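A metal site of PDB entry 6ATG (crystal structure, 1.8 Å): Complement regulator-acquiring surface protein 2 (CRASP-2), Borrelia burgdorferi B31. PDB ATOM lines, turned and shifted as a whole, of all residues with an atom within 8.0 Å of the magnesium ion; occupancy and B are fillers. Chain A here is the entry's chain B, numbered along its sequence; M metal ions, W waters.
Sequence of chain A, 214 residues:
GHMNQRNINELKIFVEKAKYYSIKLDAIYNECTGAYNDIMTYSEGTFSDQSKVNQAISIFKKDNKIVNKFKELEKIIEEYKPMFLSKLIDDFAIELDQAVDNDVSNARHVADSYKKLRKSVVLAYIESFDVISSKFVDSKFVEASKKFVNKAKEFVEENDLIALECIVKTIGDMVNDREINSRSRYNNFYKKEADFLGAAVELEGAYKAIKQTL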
ATOM      1  N   ASP A  91     -23.344 -29.652 -19.438  1.00  0.00           N
ATOM      2  CA  ASP A  91     -24.554 -28.937 -19.854  1.00  0.00           C
ATOM      3  C   ASP A  91     -24.276 -27.448 -20.023  1.00  0.00           C
ATOM      4  O   ASP A  91     -24.781 -26.816 -20.964  1.00  0.00           O
ATOM      5  CB  ASP A  91     -25.698 -29.154 -18.853  1.00  0.00           C
ATOM      6  CG  ASP A  91     -27.060 -28.796 -19.447  1.00  0.00           C
ATOM      7  OD1 ASP A  91     -27.406 -29.345 -20.526  1.00  0.00           O
ATOM      8  OD2 ASP A  91     -27.790 -27.967 -18.869  1.00  0.00           O
ATOM      9  N   ILE A  94     -22.481 -27.115 -23.318  1.00  0.00           N
ATOM     10  CA  ILE A  94     -23.410 -27.252 -24.443  1.00  0.00           C
ATOM     11  C   ILE A  94     -24.206 -25.966 -24.646  1.00  0.00           C
ATOM     12  O   ILE A  94     -24.348 -25.468 -25.773  1.00  0.00           O
ATOM     13  CB  ILE A  94     -24.343 -28.456 -24.235  1.00  0.00           C
ATOM     14  CG1 ILE A  94     -23.576 -29.767 -24.337  1.00  0.00           C
ATOM     15  CG2 ILE A  94     -25.486 -28.425 -25.262  1.00  0.00           C
ATOM     16  CD1 ILE A  94     -24.366 -30.977 -23.863  1.00  0.00           C
ATOM     17  N   GLU A  95     -24.737 -25.393 -23.554  1.00  0.00           N
ATOM     18  CA  GLU A  95     -25.494 -24.149 -23.739  1.00  0.00           C
ATOM     19  C   GLU A  95     -24.602 -23.036 -24.267  1.00  0.00           C
ATOM     20  O   GLU A  95     -25.050 -22.197 -25.056  1.00  0.00           O
ATOM     21  CB  GLU A  95     -26.166 -23.735 -22.419  1.00  0.00           C
ATOM     22  CG  GLU A  95     -27.164 -24.751 -21.858  1.00  0.00           C
ATOM     23  CD  GLU A  95     -28.367 -25.004 -22.776  1.00  0.00           C
ATOM     24  OE1 GLU A  95     -28.674 -24.157 -23.642  1.00  0.00           O
ATOM     25  OE2 GLU A  95     -29.004 -26.065 -22.602  1.00  0.00           O
ATOM     26  N   LEU A  96     -23.319 -23.023 -23.875  1.00  0.00           N
ATOM     27  CA  LEU A  96     -22.399 -22.035 -24.437  1.00  0.00           C
ATOM     28  C   LEU A  96     -22.189 -22.258 -25.934  1.00  0.00           C
ATOM     29  O   LEU A  96     -22.163 -21.303 -26.708  1.00  0.00           O
ATOM     30  CB  LEU A  96     -21.052 -22.085 -23.702  1.00  0.00           C
ATOM     31  CG  LEU A  96     -21.024 -21.537 -22.260  1.00  0.00           C
ATOM     32  CD1 LEU A  96     -19.712 -21.872 -21.568  1.00  0.00           C
ATOM     33  CD2 LEU A  96     -21.306 -20.033 -22.219  1.00  0.00           C
ATOM     34  N   GLN A  98     -24.284 -23.415 -28.032  1.00  0.00           N
ATOM     35  CA  GLN A  98     -25.464 -23.003 -28.775  1.00  0.00           C
ATOM     36  C   GLN A  98     -25.494 -21.501 -29.032  1.00  0.00           C
ATOM     37  O   GLN A  98     -26.137 -21.044 -29.989  1.00  0.00           O
ATOM     38  CB  GLN A  98     -26.736 -23.406 -28.035  1.00  0.00           C
ATOM     39  CG  GLN A  98     -26.936 -24.905 -27.860  1.00  0.00           C
ATOM     40  CD  GLN A  98     -28.183 -25.221 -27.047  1.00  0.00           C
ATOM     41  OE1 GLN A  98     -28.834 -24.318 -26.510  1.00  0.00           O
ATOM     42  NE2 GLN A  98     -28.523 -26.509 -26.966  1.00  0.00           N
ATOM     43  N   ALA A  99     -24.804 -20.706 -28.202  1.00  0.00           N
ATOM     44  CA  ALA A  99     -24.761 -19.264 -28.388  1.00  0.00           C
ATOM     45  C   ALA A  99     -23.794 -18.925 -29.510  1.00  0.00           C
ATOM     46  O   ALA A  99     -22.598 -19.200 -29.411  1.00  0.00           O
ATOM     47  CB  ALA A  99     -24.360 -18.581 -27.083  1.00  0.00           C
ATOM     48  N   SER A 105     -30.540 -15.645 -28.266  1.00  0.00           N
ATOM     49  CA  SER A 105     -31.706 -16.477 -27.994  1.00  0.00           C
ATOM     50  C   SER A 105     -31.452 -17.517 -26.906  1.00  0.00           C
ATOM     51  O   SER A 105     -32.413 -17.999 -26.289  1.00  0.00           O
ATOM     52  CB  SER A 105     -32.172 -17.182 -29.280  1.00  0.00           C
ATOM     53  OG  SER A 105     -31.127 -18.000 -29.780  1.00  0.00           O
ATOM     54  N   ASN A 106     -30.206 -17.894 -26.676  1.00  0.00           N
ATOM     55  CA  ASN A 106     -29.892 -18.908 -25.675  1.00  0.00           C
ATOM     56  C   ASN A 106     -29.391 -18.302 -24.378  1.00  0.00           C
ATOM     57  O   ASN A 106     -28.887 -19.047 -23.519  1.00  0.00           O
ATOM     58  CB  ASN A 106     -28.852 -19.897 -26.211  1.00  0.00           C
ATOM     59  CG  ASN A 106     -28.872 -21.211 -25.481  1.00  0.00           C
ATOM     60  OD1 ASN A 106     -29.927 -21.834 -25.337  1.00  0.00           O
ATOM     61  ND2 ASN A 106     -27.717 -21.649 -25.020  1.00  0.00           N
ATOM     62  N   ALA A 107     -29.526 -16.985 -24.200  1.00  0.00           N
ATOM     63  CA  ALA A 107     -28.890 -16.294 -23.089  1.00  0.00           C
ATOM     64  C   ALA A 107     -29.368 -16.807 -21.730  1.00  0.00           C
ATOM     65  O   ALA A 107     -28.558 -17.069 -20.842  1.00  0.00           O
ATOM     66  CB  ALA A 107     -29.117 -14.782 -23.202  1.00  0.00           C
ATOM     67  N   ARG A 108     -30.688 -16.928 -21.556  1.00  0.00           N
ATOM     68  CA  ARG A 108     -31.204 -17.377 -20.258  1.00  0.00           C
ATOM     69  C   ARG A 108     -30.748 -18.804 -19.948  1.00  0.00           C
ATOM     70  O   ARG A 108     -30.472 -19.136 -18.791  1.00  0.00           O
ATOM     71  CB  ARG A 108     -32.732 -17.288 -20.221  1.00  0.00           C
ATOM     72  CG  ARG A 108     -33.375 -17.760 -18.927  1.00  0.00           C
ATOM     73  CD  ARG A 108     -32.899 -16.974 -17.707  1.00  0.00           C
ATOM     74  NE  ARG A 108     -33.588 -17.395 -16.490  1.00  0.00           N
ATOM     75  CZ  ARG A 108     -34.704 -16.854 -16.015  1.00  0.00           C
ATOM     76  NH1 ARG A 108     -35.286 -15.845 -16.651  1.00  0.00           N
ATOM     77  NH2 ARG A 108     -35.247 -17.322 -14.895  1.00  0.00           N
ATOM     78  N   HIS A 109     -30.659 -19.666 -20.971  1.00  0.00           N
ATOM     79  CA  HIS A 109     -30.157 -21.022 -20.744  1.00  0.00           C
ATOM     80  C   HIS A 109     -28.711 -21.006 -20.241  1.00  0.00           C
ATOM     81  O   HIS A 109     -28.345 -21.808 -19.361  1.00  0.00           O
ATOM     82  CB  HIS A 109     -30.237 -21.839 -22.051  1.00  0.00           C
ATOM     83  CG  HIS A 109     -31.572 -22.498 -22.268  1.00  0.00           C
ATOM     84  ND1 HIS A 109     -31.806 -23.358 -23.321  1.00  0.00           N
ATOM     85  CD2 HIS A 109     -32.735 -22.428 -21.573  1.00  0.00           C
ATOM     86  CE1 HIS A 109     -33.049 -23.785 -23.265  1.00  0.00           C
ATOM     87  NE2 HIS A 109     -33.646 -23.237 -22.217  1.00  0.00           N
ATOM     88  N   VAL A 110     -27.886 -20.115 -20.796  1.00  0.00           N
ATOM     89  CA  VAL A 110     -26.508 -19.990 -20.320  1.00  0.00           C
ATOM     90  C   VAL A 110     -26.490 -19.542 -18.858  1.00  0.00           C
ATOM     91  O   VAL A 110     -25.768 -20.100 -18.019  1.00  0.00           O
ATOM     92  CB  VAL A 110     -25.727 -19.006 -21.208  1.00  0.00           C
ATOM     93  CG1 VAL A 110     -24.372 -18.680 -20.589  1.00  0.00           C
ATOM     94  CG2 VAL A 110     -25.547 -19.561 -22.631  1.00  0.00           C
HETATM   95 MG    MG M   1     -30.321 -23.905 -25.066  1.00  0.00          MG
HETATM   96  O   HOH W   1     -31.726 -23.844 -26.361  1.00  0.00           O
HETATM   97  O   HOH W   2     -30.709 -26.002 -24.838  1.00  0.00           O
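Within 4 Å of the magnesium ion: Glu 95, Gln 98, Asn 106 and His 109.
Water W2 bridges OE2 of Glu 95 and NE2 of Gln 98.
The magnesium ion is bound by water W1 (1.9 Å), the side-chain amide oxygen of Gln 98 (2.1 Å), the side-chain amide oxygen of Asn 106 (2.1 Å), water W2 (2.1 Å), the side-chain carboxylate of Glu 95 (2.2 Å) and a ring nitrogen (ND1) of His 109 (2.4 Å). The magnesium ion has six donor atoms within binding distance.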
